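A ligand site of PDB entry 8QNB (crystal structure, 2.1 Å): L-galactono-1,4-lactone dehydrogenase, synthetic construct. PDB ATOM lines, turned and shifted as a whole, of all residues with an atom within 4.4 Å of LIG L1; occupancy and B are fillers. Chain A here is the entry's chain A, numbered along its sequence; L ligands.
O5 of LIG L1 lies within hydrogen-bond range of NH2 of Arg 50, at 3.2 Å.
O14 of LIG L1 lies within hydrogen-bond range of N of Leu 56 (2.9 Å).
The backbone carbonyl oxygen of Gly 122 lies within hydrogen-bond range of an oxygen (O11) of LIG L1, at 2.7 Å.
N of His 129 lies within hydrogen-bond range of O7 of LIG L1.
O of Val 179 sits at hydrogen-bond distance from N3 of LIG L1 (3.1 Å).
NE2 of Gln 118 is in hydrogen-bond range of O9 of LIG L1 (3.0 Å).
O1 of LIG L1 sits at hydrogen-bond distance from OG of Ser 57 (2.7 Å).
The backbone carbonyl oxygen of Cys 340 lies close to an oxygen (O3) of LG2 L2, at 3.3 Å.
O8 of LIG L1 sits at hydrogen-bond distance from NH1 of Arg 388.
The guanidinium group (NH2) of Arg 388 lies within hydrogen-bond range of an oxygen (O6) of LG2 L2 (3.0 Å).
The backbone NH (N) of Ser 54 lies within hydrogen-bond range of an oxygen (O13) of LIG L1, at 2.9 Å.
A nitrogen (N4) of LIG L1 sits at hydrogen-bond distance from the backbone NH (N) of Val 179.
The backbone carbonyl oxygen (O) of Leu 173 is in hydrogen-bond range of an oxygen (O5) of LIG L1 (3.1 Å).
OG of Ser 114 is in hydrogen-bond range of O5 of LG2 L2 (2.9 Å).
O6 of LIG L1 lies within hydrogen-bond range of O of Pro 51, 2.7 Å away.
An oxygen (O2) of LIG L1 lies within hydrogen-bond range of the backbone NH of Gly 55 (3.0 Å).
O2 of LIG L1 is in hydrogen-bond range of N of Gly 53 (2.7 Å).
An oxygen (O13) of LIG L1 is in hydrogen-bond range of the backbone NH of Gln 119 (2.8 Å).
An oxygen (O1) of LIG L1 lies close to the backbone NH (N) of Ser 57, 3.2 Å away.
The backbone NH (N) of Ser 114 lies within hydrogen-bond range of an oxygen (O8) of LIG L1, 2.9 Å away.
N8 of LIG L1 lies within hydrogen-bond range of OG of Ser 114 (2.7 Å).
O of His 129 is in hydrogen-bond range of N7 of LIG L1, at 2.8 Å.
A ring nitrogen (NE2) of His 453 sits at hydrogen-bond distance from an oxygen (O7) of LIG L1, at 2.8 Å.
O6 of LG2 L2 lies close to N8 of LIG L1 (3.4 Å).
The backbone NH (N) of Ala 128 sits at hydrogen-bond distance from the backbone carbonyl oxygen (O) of Phe 123 (3.3 Å).
N of Gly 174 sits at hydrogen-bond distance from OE1 of Gln 125 (2.8 Å).
The side-chain amide oxygen (OE1) of Gln 125 sits at hydrogen-bond distance from the backbone NH (N) of Leu 173, at 3.0 Å.
ND1 of His 453 lies within hydrogen-bond range of N of Ala 455, at 3.2 Å.
The side-chain sulfur (SG) of Cys 340 sits at hydrogen-bond distance from the side-chain hydroxyl (OG) of Ser 114.
NE2 of Gln 119 lies close to O of Gly 53 (3.5 Å).
The backbone carbonyl oxygen (O) of Leu 173 sits at hydrogen-bond distance from the guanidinium group (NH2) of Arg 50, 2.7 Å away.
The side-chain amide oxygen (OE1) of Gln 118 sits close to the backbone carbonyl oxygen (O) of Ile 115 (2.9 Å).
Trp 15 touches LIG L1.
C of Val 52 touches N2 of LIG L1, at 3.7 Å.
CD of Pro 58 touches O10 of LIG L1, 3.9 Å away.
CD2 of Leu 61 touches O5 of LIG L1, 3.3 Å away.
Ala 62 touches LIG L1.
Ala 91 touches LIG L1 (CB to N3, 3.96 Å).
Ala 113 touches LIG L1.
Ile 115 touches LIG L1.
Gln 125 touches LIG L1.
Val 126 touches LIG L1.
CA of Ala 128 touches O7 of LIG L1, at 3.0 Å.
CA of Gly 174 touches N5 of LIG L1, 3.3 Å away.
Gly 177 touches LIG L1 (O to C9, 3.3 Å).
CA of Val 178 touches N4 of LIG L1, at 3.6 Å.
Ala 455 touches LIG L1 (CB to O10, 3.1 Å).
The nearest printed residue that does not touch LIG L1 is Gly 121 (4.03 Å).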
ATOM      1  N   TRP A  15     -14.748  -8.538  33.594  1.00  0.00           N
ATOM      2  CA  TRP A  15     -15.112  -8.688  35.024  1.00  0.00           C
ATOM      3  C   TRP A  15     -14.871  -7.363  35.751  1.00  0.00           C
ATOM      4  O   TRP A  15     -15.743  -6.940  36.500  1.00  0.00           O
ATOM      5  CB  TRP A  15     -14.300  -9.850  35.625  1.00  0.00           C
ATOM      6  CG  TRP A  15     -14.829 -10.393  36.917  1.00  0.00           C
ATOM      7  CD1 TRP A  15     -15.791 -11.347  37.076  1.00  0.00           C
ATOM      8  CD2 TRP A  15     -14.370 -10.054  38.243  1.00  0.00           C
ATOM      9  NE1 TRP A  15     -15.966 -11.626  38.418  1.00  0.00           N
ATOM     10  CE2 TRP A  15     -15.115 -10.834  39.148  1.00  0.00           C
ATOM     11  CE3 TRP A  15     -13.400  -9.183  38.733  1.00  0.00           C
ATOM     12  CZ2 TRP A  15     -14.935 -10.758  40.526  1.00  0.00           C
ATOM     13  CZ3 TRP A  15     -13.214  -9.094  40.095  1.00  0.00           C
ATOM     14  CH2 TRP A  15     -13.961  -9.886  40.982  1.00  0.00           C
ATOM     15  N   ARG A  50     -14.176 -13.404  16.118  1.00  0.00           N
ATOM     16  CA  ARG A  50     -13.340 -13.856  17.236  1.00  0.00           C
ATOM     17  C   ARG A  50     -14.208 -14.672  18.201  1.00  0.00           C
ATOM     18  O   ARG A  50     -15.303 -14.264  18.576  1.00  0.00           O
ATOM     19  CB  ARG A  50     -12.652 -12.692  17.932  1.00  0.00           C
ATOM     20  CG  ARG A  50     -11.598 -13.190  18.916  1.00  0.00           C
ATOM     21  CD  ARG A  50     -10.258 -12.532  18.737  1.00  0.00           C
ATOM     22  NE  ARG A  50      -9.361 -12.867  19.832  1.00  0.00           N
ATOM     23  CZ  ARG A  50      -8.689 -14.000  19.953  1.00  0.00           C
ATOM     24  NH1 ARG A  50      -8.803 -14.951  19.044  1.00  0.00           N
ATOM     25  NH2 ARG A  50      -7.895 -14.155  20.984  1.00  0.00           N
ATOM     26  N   PRO A  51     -13.770 -15.883  18.596  1.00  0.00           N
ATOM     27  CA  PRO A  51     -14.491 -16.641  19.620  1.00  0.00           C
ATOM     28  C   PRO A  51     -14.418 -15.876  20.947  1.00  0.00           C
ATOM     29  O   PRO A  51     -13.429 -15.235  21.268  1.00  0.00           O
ATOM     30  CB  PRO A  51     -13.793 -17.999  19.689  1.00  0.00           C
ATOM     31  CG  PRO A  51     -12.855 -18.035  18.509  1.00  0.00           C
ATOM     32  CD  PRO A  51     -12.563 -16.591  18.153  1.00  0.00           C
ATOM     33  N   VAL A  52     -15.544 -15.887  21.657  1.00  0.00           N
ATOM     34  CA  VAL A  52     -15.686 -15.269  22.996  1.00  0.00           C
ATOM     35  C   VAL A  52     -16.383 -16.311  23.873  1.00  0.00           C
ATOM     36  O   VAL A  52     -17.263 -17.007  23.364  1.00  0.00           O
ATOM     37  CB  VAL A  52     -16.418 -13.908  22.905  1.00  0.00           C
ATOM     38  CG1 VAL A  52     -17.837 -14.044  22.357  1.00  0.00           C
ATOM     39  CG2 VAL A  52     -16.436 -13.200  24.249  1.00  0.00           C
ATOM     40  N   GLY A  53     -15.918 -16.483  25.105  1.00  0.00           N
ATOM     41  CA  GLY A  53     -16.639 -17.241  26.129  1.00  0.00           C
ATOM     42  C   GLY A  53     -17.434 -16.256  26.960  1.00  0.00           C
ATOM     43  O   GLY A  53     -18.234 -15.488  26.351  1.00  0.00           O
ATOM     44  N   SER A  54     -17.187 -16.210  28.268  1.00  0.00           N
ATOM     45  CA  SER A  54     -17.949 -15.353  29.214  1.00  0.00           C
ATOM     46  C   SER A  54     -17.420 -13.914  29.147  1.00  0.00           C
ATOM     47  O   SER A  54     -18.000 -13.051  29.788  1.00  0.00           O
ATOM     48  CB  SER A  54     -17.917 -15.900  30.610  1.00  0.00           C
ATOM     49  OG  SER A  54     -18.412 -17.220  30.640  1.00  0.00           O
ATOM     50  N   GLY A  55     -16.337 -13.682  28.399  1.00  0.00           N
ATOM     51  CA  GLY A  55     -15.773 -12.339  28.181  1.00  0.00           C
ATOM     52  C   GLY A  55     -15.053 -11.794  29.404  1.00  0.00           C
ATOM     53  O   GLY A  55     -14.918 -10.549  29.483  1.00  0.00           O
ATOM     54  N   LEU A  56     -14.540 -12.663  30.291  1.00  0.00           N
ATOM     55  CA  LEU A  56     -14.068 -12.278  31.649  1.00  0.00           C
ATOM     56  C   LEU A  56     -12.606 -11.848  31.602  1.00  0.00           C
ATOM     57  O   LEU A  56     -12.228 -11.028  32.478  1.00  0.00           O
ATOM     58  CB  LEU A  56     -14.238 -13.432  32.639  1.00  0.00           C
ATOM     59  CG  LEU A  56     -15.669 -13.920  32.861  1.00  0.00           C
ATOM     60  CD1 LEU A  56     -15.696 -15.096  33.809  1.00  0.00           C
ATOM     61  CD2 LEU A  56     -16.595 -12.809  33.362  1.00  0.00           C
ATOM     62  N   SER A  57     -11.829 -12.339  30.625  1.00  0.00           N
ATOM     63  CA  SER A  57     -10.368 -12.106  30.566  1.00  0.00           C
ATOM     64  C   SER A  57     -10.049 -10.679  30.986  1.00  0.00           C
ATOM     65  O   SER A  57     -10.570  -9.727  30.416  1.00  0.00           O
ATOM     66  CB  SER A  57      -9.823 -12.395  29.216  1.00  0.00           C
ATOM     67  OG  SER A  57      -9.757 -13.791  29.014  1.00  0.00           O
ATOM     68  N   PRO A  58      -9.188 -10.484  32.015  1.00  0.00           N
ATOM     69  CA  PRO A  58      -8.725  -9.146  32.395  1.00  0.00           C
ATOM     70  C   PRO A  58      -8.196  -8.288  31.236  1.00  0.00           C
ATOM     71  O   PRO A  58      -8.367  -7.102  31.290  1.00  0.00           O
ATOM     72  CB  PRO A  58      -7.623  -9.468  33.409  1.00  0.00           C
ATOM     73  CG  PRO A  58      -8.150 -10.713  34.082  1.00  0.00           C
ATOM     74  CD  PRO A  58      -8.740 -11.529  32.951  1.00  0.00           C
ATOM     75  N   LEU A  61      -8.811 -10.264  25.757  1.00  0.00           N
ATOM     76  CA  LEU A  61      -8.234 -11.158  24.725  1.00  0.00           C
ATOM     77  C   LEU A  61      -9.225 -11.515  23.594  1.00  0.00           C
ATOM     78  O   LEU A  61      -8.776 -11.611  22.391  1.00  0.00           O
ATOM     79  CB  LEU A  61      -7.757 -12.450  25.382  1.00  0.00           C
ATOM     80  CG  LEU A  61      -6.984 -13.393  24.469  1.00  0.00           C
ATOM     81  CD1 LEU A  61      -5.755 -12.671  23.931  1.00  0.00           C
ATOM     82  CD2 LEU A  61      -6.578 -14.649  25.219  1.00  0.00           C
ATOM     83  N   ALA A  62     -10.481 -11.783  23.966  1.00  0.00           N
ATOM     84  CA  ALA A  62     -11.556 -12.310  23.093  1.00  0.00           C
ATOM     85  C   ALA A  62     -12.279 -11.184  22.321  1.00  0.00           C
ATOM     86  O   ALA A  62     -13.150 -11.531  21.506  1.00  0.00           O
ATOM     87  CB  ALA A  62     -12.554 -13.073  23.929  1.00  0.00           C
ATOM     88  N   LEU A  71     -20.507 -19.289  22.199  1.00  0.00           N
ATOM     89  CA  LEU A  71     -21.199 -20.603  22.201  1.00  0.00           C
ATOM     90  C   LEU A  71     -21.987 -20.778  23.489  1.00  0.00           C
ATOM     91  O   LEU A  71     -22.360 -21.940  23.811  1.00  0.00           O
ATOM     92  CB  LEU A  71     -20.199 -21.748  22.004  1.00  0.00           C
ATOM     93  CG  LEU A  71     -19.430 -21.800  20.681  1.00  0.00           C
ATOM     94  CD1 LEU A  71     -19.099 -23.238  20.311  1.00  0.00           C
ATOM     95  CD2 LEU A  71     -20.192 -21.161  19.538  1.00  0.00           C
ATOM     96  N   ALA A  91     -18.399 -26.587  24.388  1.00  0.00           N
ATOM     97  CA  ALA A  91     -17.399 -25.573  24.823  1.00  0.00           C
ATOM     98  C   ALA A  91     -18.079 -24.442  25.614  1.00  0.00           C
ATOM     99  O   ALA A  91     -17.418 -23.926  26.539  1.00  0.00           O
ATOM    100  CB  ALA A  91     -16.656 -25.053  23.624  1.00  0.00           C
ATOM    101  N   ALA A 113      -9.999 -22.807  38.951  1.00  0.00           N
ATOM    102  CA  ALA A 113      -9.531 -21.420  39.130  1.00  0.00           C
ATOM    103  C   ALA A 113     -10.248 -20.794  40.352  1.00  0.00           C
ATOM    104  O   ALA A 113     -11.075 -21.466  40.989  1.00  0.00           O
ATOM    105  CB  ALA A 113      -9.766 -20.677  37.846  1.00  0.00           C
ATOM    106  N   SER A 114      -9.890 -19.550  40.705  1.00  0.00           N
ATOM    107  CA  SER A 114     -10.483 -18.782  41.830  1.00  0.00           C
ATOM    108  C   SER A 114     -11.950 -18.466  41.537  1.00  0.00           C
ATOM    109  O   SER A 114     -12.685 -18.238  42.520  1.00  0.00           O
ATOM    110  CB  SER A 114      -9.677 -17.551  42.146  1.00  0.00           C
ATOM    111  OG  SER A 114      -9.441 -16.758  40.993  1.00  0.00           O
ATOM    112  N   ILE A 115     -12.386 -18.485  40.277  1.00  0.00           N
ATOM    113  CA  ILE A 115     -13.842 -18.438  39.900  1.00  0.00           C
ATOM    114  C   ILE A 115     -14.127 -19.524  38.868  1.00  0.00           C
ATOM    115  O   ILE A 115     -13.169 -20.095  38.322  1.00  0.00           O
ATOM    116  CB  ILE A 115     -14.263 -17.053  39.369  1.00  0.00           C
ATOM    117  CG1 ILE A 115     -13.447 -16.661  38.132  1.00  0.00           C
ATOM    118  CG2 ILE A 115     -14.187 -16.017  40.474  1.00  0.00           C
ATOM    119  CD1 ILE A 115     -14.038 -15.519  37.329  1.00  0.00           C
ATOM    120  N   GLN A 118     -16.086 -18.891  33.950  1.00  0.00           N
ATOM    121  CA  GLN A 118     -15.401 -19.082  32.637  1.00  0.00           C
ATOM    122  C   GLN A 118     -16.127 -20.154  31.818  1.00  0.00           C
ATOM    123  O   GLN A 118     -16.505 -21.184  32.394  1.00  0.00           O
ATOM    124  CB  GLN A 118     -13.987 -19.671  32.716  1.00  0.00           C
ATOM    125  CG  GLN A 118     -12.972 -18.864  33.517  1.00  0.00           C
ATOM    126  CD  GLN A 118     -12.947 -19.265  34.976  1.00  0.00           C
ATOM    127  OE1 GLN A 118     -13.895 -19.836  35.494  1.00  0.00           O
ATOM    128  NE2 GLN A 118     -11.867 -18.924  35.651  1.00  0.00           N
ATOM    129  N   GLN A 119     -16.260 -19.983  30.512  1.00  0.00           N
ATOM    130  CA  GLN A 119     -16.727 -21.103  29.651  1.00  0.00           C
ATOM    131  C   GLN A 119     -15.594 -22.135  29.520  1.00  0.00           C
ATOM    132  O   GLN A 119     -14.412 -21.742  29.673  1.00  0.00           O
ATOM    133  CB  GLN A 119     -17.228 -20.581  28.300  1.00  0.00           C
ATOM    134  CG  GLN A 119     -18.628 -20.007  28.367  1.00  0.00           C
ATOM    135  CD  GLN A 119     -19.036 -19.504  27.014  1.00  0.00           C
ATOM    136  OE1 GLN A 119     -18.587 -20.010  25.994  1.00  0.00           O
ATOM    137  NE2 GLN A 119     -19.887 -18.497  26.996  1.00  0.00           N
ATOM    138  N   GLY A 121     -14.409 -23.514  26.841  1.00  0.00           N
ATOM    139  CA  GLY A 121     -13.549 -23.041  25.740  1.00  0.00           C
ATOM    140  C   GLY A 121     -12.566 -21.973  26.198  1.00  0.00           C
ATOM    141  O   GLY A 121     -11.345 -22.106  25.912  1.00  0.00           O
ATOM    142  N   GLY A 122     -13.067 -20.926  26.837  1.00  0.00           N
ATOM    143  CA  GLY A 122     -12.237 -19.791  27.275  1.00  0.00           C
ATOM    144  C   GLY A 122     -11.272 -20.219  28.368  1.00  0.00           C
ATOM    145  O   GLY A 122     -10.174 -19.646  28.484  1.00  0.00           O
ATOM    146  N   PHE A 123     -11.674 -21.198  29.159  1.00  0.00           N
ATOM    147  CA  PHE A 123     -10.843 -21.786  30.231  1.00  0.00           C
ATOM    148  C   PHE A 123      -9.590 -22.460  29.643  1.00  0.00           C
ATOM    149  O   PHE A 123      -8.480 -22.126  30.083  1.00  0.00           O
ATOM    150  CB  PHE A 123     -11.716 -22.736  31.027  1.00  0.00           C
ATOM    151  CG  PHE A 123     -11.211 -23.025  32.417  1.00  0.00           C
ATOM    152  CD1 PHE A 123     -10.816 -21.986  33.249  1.00  0.00           C
ATOM    153  CD2 PHE A 123     -11.166 -24.323  32.903  1.00  0.00           C
ATOM    154  CE1 PHE A 123     -10.385 -22.256  34.544  1.00  0.00           C
ATOM    155  CE2 PHE A 123     -10.739 -24.576  34.192  1.00  0.00           C
ATOM    156  CZ  PHE A 123     -10.339 -23.544  35.001  1.00  0.00           C
ATOM    157  N   GLN A 125      -8.383 -22.267  26.385  1.00  0.00           N
ATOM    158  CA  GLN A 125      -7.677 -21.559  25.282  1.00  0.00           C
ATOM    159  C   GLN A 125      -6.585 -20.616  25.835  1.00  0.00           C
ATOM    160  O   GLN A 125      -5.741 -20.174  25.045  1.00  0.00           O
ATOM    161  CB  GLN A 125      -8.662 -20.792  24.385  1.00  0.00           C
ATOM    162  CG  GLN A 125      -9.459 -21.666  23.443  1.00  0.00           C
ATOM    163  CD  GLN A 125      -8.596 -22.269  22.361  1.00  0.00           C
ATOM    164  OE1 GLN A 125      -8.016 -21.573  21.528  1.00  0.00           O
ATOM    165  NE2 GLN A 125      -8.446 -23.583  22.434  1.00  0.00           N
ATOM    166  N   VAL A 126      -6.592 -20.313  27.136  1.00  0.00           N
ATOM    167  CA  VAL A 126      -5.570 -19.440  27.801  1.00  0.00           C
ATOM    168  C   VAL A 126      -4.669 -20.265  28.721  1.00  0.00           C
ATOM    169  O   VAL A 126      -3.694 -19.680  29.282  1.00  0.00           O
ATOM    170  CB  VAL A 126      -6.250 -18.291  28.551  1.00  0.00           C
ATOM    171  CG1 VAL A 126      -7.246 -17.586  27.628  1.00  0.00           C
ATOM    172  CG2 VAL A 126      -6.921 -18.736  29.855  1.00  0.00           C
ATOM    173  N   ALA A 128      -5.626 -21.844  31.624  1.00  0.00           N
ATOM    174  CA  ALA A 128      -6.002 -21.458  33.009  1.00  0.00           C
ATOM    175  C   ALA A 128      -5.584 -22.569  33.968  1.00  0.00           C
ATOM    176  O   ALA A 128      -5.474 -23.704  33.526  1.00  0.00           O
ATOM    177  CB  ALA A 128      -7.487 -21.209  33.124  1.00  0.00           C
ATOM    178  N   HIS A 129      -5.389 -22.232  35.230  1.00  0.00           N
ATOM    179  CA  HIS A 129      -4.749 -23.108  36.234  1.00  0.00           C
ATOM    180  C   HIS A 129      -5.294 -22.806  37.620  1.00  0.00           C
ATOM    181  O   HIS A 129      -5.814 -21.688  37.847  1.00  0.00           O
ATOM    182  CB  HIS A 129      -3.216 -22.920  36.216  1.00  0.00           C
ATOM    183  CG  HIS A 129      -2.824 -21.598  36.792  1.00  0.00           C
ATOM    184  ND1 HIS A 129      -2.619 -21.432  38.147  1.00  0.00           N
ATOM    185  CD2 HIS A 129      -2.684 -20.383  36.225  1.00  0.00           C
ATOM    186  CE1 HIS A 129      -2.341 -20.164  38.382  1.00  0.00           C
ATOM    187  NE2 HIS A 129      -2.378 -19.507  37.216  1.00  0.00           N
ATOM    188  N   LEU A 173      -5.746 -19.741  22.090  1.00  0.00           N
ATOM    189  CA  LEU A 173      -6.077 -18.302  22.216  1.00  0.00           C
ATOM    190  C   LEU A 173      -7.157 -17.912  21.190  1.00  0.00           C
ATOM    191  O   LEU A 173      -7.128 -16.777  20.729  1.00  0.00           O
ATOM    192  CB  LEU A 173      -4.835 -17.437  21.992  1.00  0.00           C
ATOM    193  CG  LEU A 173      -3.558 -17.847  22.720  1.00  0.00           C
ATOM    194  CD1 LEU A 173      -2.437 -16.880  22.376  1.00  0.00           C
ATOM    195  CD2 LEU A 173      -3.767 -17.883  24.207  1.00  0.00           C
ATOM    196  N   GLY A 174      -8.032 -18.848  20.830  1.00  0.00           N
ATOM    197  CA  GLY A 174      -9.098 -18.669  19.816  1.00  0.00           C
ATOM    198  C   GLY A 174      -8.589 -18.348  18.414  1.00  0.00           C
ATOM    199  O   GLY A 174      -9.412 -17.921  17.610  1.00  0.00           O
ATOM    200  N   GLY A 177      -9.368 -21.891  15.631  1.00  0.00           N
ATOM    201  CA  GLY A 177     -10.697 -22.479  15.396  1.00  0.00           C
ATOM    202  C   GLY A 177     -11.630 -22.252  16.567  1.00  0.00           C
ATOM    203  O   GLY A 177     -11.155 -21.873  17.675  1.00  0.00           O
ATOM    204  N   VAL A 178     -12.923 -22.474  16.308  1.00  0.00           N
ATOM    205  CA  VAL A 178     -13.989 -22.346  17.326  1.00  0.00           C
ATOM    206  C   VAL A 178     -14.167 -23.743  17.912  1.00  0.00           C
ATOM    207  O   VAL A 178     -14.687 -24.629  17.198  1.00  0.00           O
ATOM    208  CB  VAL A 178     -15.288 -21.770  16.748  1.00  0.00           C
ATOM    209  CG1 VAL A 178     -16.316 -21.571  17.843  1.00  0.00           C
ATOM    210  CG2 VAL A 178     -15.049 -20.475  15.980  1.00  0.00           C
ATOM    211  N   VAL A 179     -13.773 -23.903  19.165  1.00  0.00           N
ATOM    212  CA  VAL A 179     -13.976 -25.144  19.946  1.00  0.00           C
ATOM    213  C   VAL A 179     -15.480 -25.296  20.189  1.00  0.00           C
ATOM    214  O   VAL A 179     -16.114 -24.314  20.613  1.00  0.00           O
ATOM    215  CB  VAL A 179     -13.197 -25.145  21.266  1.00  0.00           C
ATOM    216  CG1 VAL A 179     -13.330 -26.480  21.963  1.00  0.00           C
ATOM    217  CG2 VAL A 179     -11.736 -24.806  21.048  1.00  0.00           C
ATOM    218  N   CYS A 340     -12.247 -12.894  45.255  1.00  0.00           N
ATOM    219  CA  CYS A 340     -11.164 -12.137  44.568  1.00  0.00           C
ATOM    220  C   CYS A 340     -11.337 -10.634  44.837  1.00  0.00           C
ATOM    221  O   CYS A 340     -10.401  -9.861  44.546  1.00  0.00           O
ATOM    222  CB  CYS A 340     -11.136 -12.432  43.078  1.00  0.00           C
ATOM    223  SG  CYS A 340     -10.989 -14.203  42.738  1.00  0.00           S
ATOM    224  N   ARG A 388       0.859 -19.474  43.587  1.00  0.00           N
ATOM    225  CA  ARG A 388       0.336 -20.836  43.385  1.00  0.00           C
ATOM    226  C   ARG A 388       1.402 -21.661  42.655  1.00  0.00           C
ATOM    227  O   ARG A 388       2.491 -21.108  42.345  1.00  0.00           O
ATOM    228  CB  ARG A 388      -0.992 -20.684  42.648  1.00  0.00           C
ATOM    229  CG  ARG A 388      -2.034 -19.993  43.516  1.00  0.00           C
ATOM    230  CD  ARG A 388      -3.365 -19.980  42.791  1.00  0.00           C
ATOM    231  NE  ARG A 388      -3.310 -18.959  41.753  1.00  0.00           N
ATOM    232  CZ  ARG A 388      -4.318 -18.641  40.942  1.00  0.00           C
ATOM    233  NH1 ARG A 388      -5.461 -19.295  40.998  1.00  0.00           N
ATOM    234  NH2 ARG A 388      -4.154 -17.662  40.061  1.00  0.00           N
ATOM    235  N   HIS A 453       0.471 -15.000  31.936  1.00  0.00           N
ATOM    236  CA  HIS A 453      -0.895 -15.535  31.716  1.00  0.00           C
ATOM    237  C   HIS A 453      -1.490 -14.827  30.506  1.00  0.00           C
ATOM    238  O   HIS A 453      -1.496 -13.558  30.488  1.00  0.00           O
ATOM    239  CB  HIS A 453      -1.733 -15.297  32.985  1.00  0.00           C
ATOM    240  CG  HIS A 453      -2.919 -16.177  33.080  1.00  0.00           C
ATOM    241  ND1 HIS A 453      -3.980 -16.082  32.197  1.00  0.00           N
ATOM    242  CD2 HIS A 453      -3.223 -17.153  33.963  1.00  0.00           C
ATOM    243  CE1 HIS A 453      -4.892 -16.974  32.538  1.00  0.00           C
ATOM    244  NE2 HIS A 453      -4.454 -17.644  33.626  1.00  0.00           N
ATOM    245  N   ALA A 455      -4.555 -14.347  29.562  1.00  0.00           N
ATOM    246  CA  ALA A 455      -5.748 -13.525  29.894  1.00  0.00           C
ATOM    247  C   ALA A 455      -5.342 -12.238  30.610  1.00  0.00           C
ATOM    248  O   ALA A 455      -6.242 -11.414  30.882  1.00  0.00           O
ATOM    249  CB  ALA A 455      -6.704 -14.316  30.752  1.00  0.00           C
HETATM  250  P1  LIG L   1     -12.897 -15.276  27.286  1.00  0.00           P
HETATM  251  O1  LIG L   1     -12.172 -14.157  27.956  1.00  0.00           O
HETATM  252  O2  LIG L   1     -14.282 -15.055  26.760  1.00  0.00           O
HETATM  253  O3  LIG L   1     -11.999 -15.853  26.099  1.00  0.00           O
HETATM  254  C1  LIG L   1     -10.672 -16.339  26.451  1.00  0.00           C
HETATM  255  C2  LIG L   1      -9.976 -16.887  25.236  1.00  0.00           C
HETATM  256  O4  LIG L   1     -10.655 -18.075  24.749  1.00  0.00           O
HETATM  257  C3  LIG L   1      -9.909 -15.946  24.017  1.00  0.00           C
HETATM  258  O5  LIG L   1      -8.707 -16.215  23.316  1.00  0.00           O
HETATM  259  C4  LIG L   1     -11.092 -16.399  23.151  1.00  0.00           C
HETATM  260  O6  LIG L   1     -10.925 -16.030  21.806  1.00  0.00           O
HETATM  261  C5  LIG L   1     -11.017 -17.902  23.389  1.00  0.00           C
HETATM  262  N1  LIG L   1     -12.253 -18.602  23.224  1.00  0.00           N
HETATM  263  C6  LIG L   1     -13.351 -18.502  24.023  1.00  0.00           C
HETATM  264  N2  LIG L   1     -14.298 -19.338  23.688  1.00  0.00           N
HETATM  265  C7  LIG L   1     -13.761 -20.058  22.628  1.00  0.00           C
HETATM  266  C8  LIG L   1     -14.267 -21.082  21.830  1.00  0.00           C
HETATM  267  N3  LIG L   1     -15.451 -21.638  22.031  1.00  0.00           N
HETATM  268  N4  LIG L   1     -13.453 -21.568  20.846  1.00  0.00           N
HETATM  269  C9  LIG L   1     -12.249 -21.021  20.682  1.00  0.00           C
HETATM  270  N5  LIG L   1     -11.659 -20.050  21.383  1.00  0.00           N
HETATM  271  C10 LIG L   1     -12.487 -19.617  22.346  1.00  0.00           C
HETATM  272  N6  LIG L   1      -7.299 -17.805  35.323  1.00  0.00           N
HETATM  273  C11 LIG L   1      -6.575 -18.777  35.892  1.00  0.00           C
HETATM  274  O7  LIG L   1      -5.784 -19.448  35.230  1.00  0.00           O
HETATM  275  N7  LIG L   1      -6.676 -19.062  37.242  1.00  0.00           N
HETATM  276  C12 LIG L   1      -7.510 -18.361  38.070  1.00  0.00           C
HETATM  277  O8  LIG L   1      -7.585 -18.664  39.248  1.00  0.00           O
HETATM  278  C13 LIG L   1      -8.239 -17.285  37.516  1.00  0.00           C
HETATM  279  N8  LIG L   1      -9.017 -16.582  38.297  1.00  0.00           N
HETATM  280  C14 LIG L   1      -9.656 -15.517  37.747  1.00  0.00           C
HETATM  281  C15 LIG L   1     -10.439 -14.706  38.590  1.00  0.00           C
HETATM  282  C16 LIG L   1     -11.128 -13.625  38.116  1.00  0.00           C
HETATM  283  C17 LIG L   1     -11.941 -12.777  39.067  1.00  0.00           C
HETATM  284  C18 LIG L   1     -11.053 -13.308  36.729  1.00  0.00           C
HETATM  285  C19 LIG L   1     -11.789 -12.120  36.179  1.00  0.00           C
HETATM  286  C20 LIG L   1     -10.311 -14.108  35.888  1.00  0.00           C
HETATM  287  C21 LIG L   1      -9.592 -15.219  36.364  1.00  0.00           C
HETATM  288  N9  LIG L   1      -8.792 -16.030  35.564  1.00  0.00           N
HETATM  289  C22 LIG L   1      -8.063 -17.068  36.102  1.00  0.00           C
HETATM  290  C23 LIG L   1      -8.675 -15.795  34.115  1.00  0.00           C
HETATM  291  C24 LIG L   1      -9.726 -16.604  33.385  1.00  0.00           C
HETATM  292  O9  LIG L   1      -9.716 -17.993  33.736  1.00  0.00           O
HETATM  293  C25 LIG L   1      -9.522 -16.455  31.884  1.00  0.00           C
HETATM  294  O10 LIG L   1      -9.625 -15.081  31.598  1.00  0.00           O
HETATM  295  C26 LIG L   1     -10.517 -17.220  31.017  1.00  0.00           C
HETATM  296  O11 LIG L   1     -10.009 -17.219  29.679  1.00  0.00           O
HETATM  297  C27 LIG L   1     -11.871 -16.575  31.046  1.00  0.00           C
HETATM  298  O12 LIG L   1     -12.834 -17.476  30.444  1.00  0.00           O
HETATM  299  P2  LIG L   1     -13.917 -16.851  29.433  1.00  0.00           P
HETATM  300  O13 LIG L   1     -14.979 -17.864  29.142  1.00  0.00           O
HETATM  301  O14 LIG L   1     -14.356 -15.544  29.996  1.00  0.00           O
HETATM  302  O15 LIG L   1     -12.976 -16.596  28.176  1.00  0.00           O
HETATM  303  O1  LG2 L   2      -7.221 -13.076  37.867  1.00  0.00           O
HETATM  304  C1  LG2 L   2      -7.183 -13.438  39.021  1.00  0.00           C
HETATM  305  O2  LG2 L   2      -7.481 -12.600  40.047  1.00  0.00           O
HETATM  306  C2  LG2 L   2      -7.491 -13.354  41.321  1.00  0.00           C
HETATM  307  C3  LG2 L   2      -7.132 -12.407  42.448  1.00  0.00           C
HETATM  308  O3  LG2 L   2      -8.112 -11.452  42.751  1.00  0.00           O
HETATM  309  C4  LG2 L   2      -6.380 -12.974  43.646  1.00  0.00           C
HETATM  310  O4  LG2 L   2      -6.198 -12.007  44.685  1.00  0.00           O
HETATM  311  C5  LG2 L   2      -6.548 -14.530  41.052  1.00  0.00           C
HETATM  312  O5  LG2 L   2      -6.858 -15.675  41.847  1.00  0.00           O
HETATM  313  C6  LG2 L   2      -6.890 -14.826  39.584  1.00  0.00           C
HETATM  314  O6  LG2 L   2      -5.871 -15.507  38.883  1.00  0.00           O
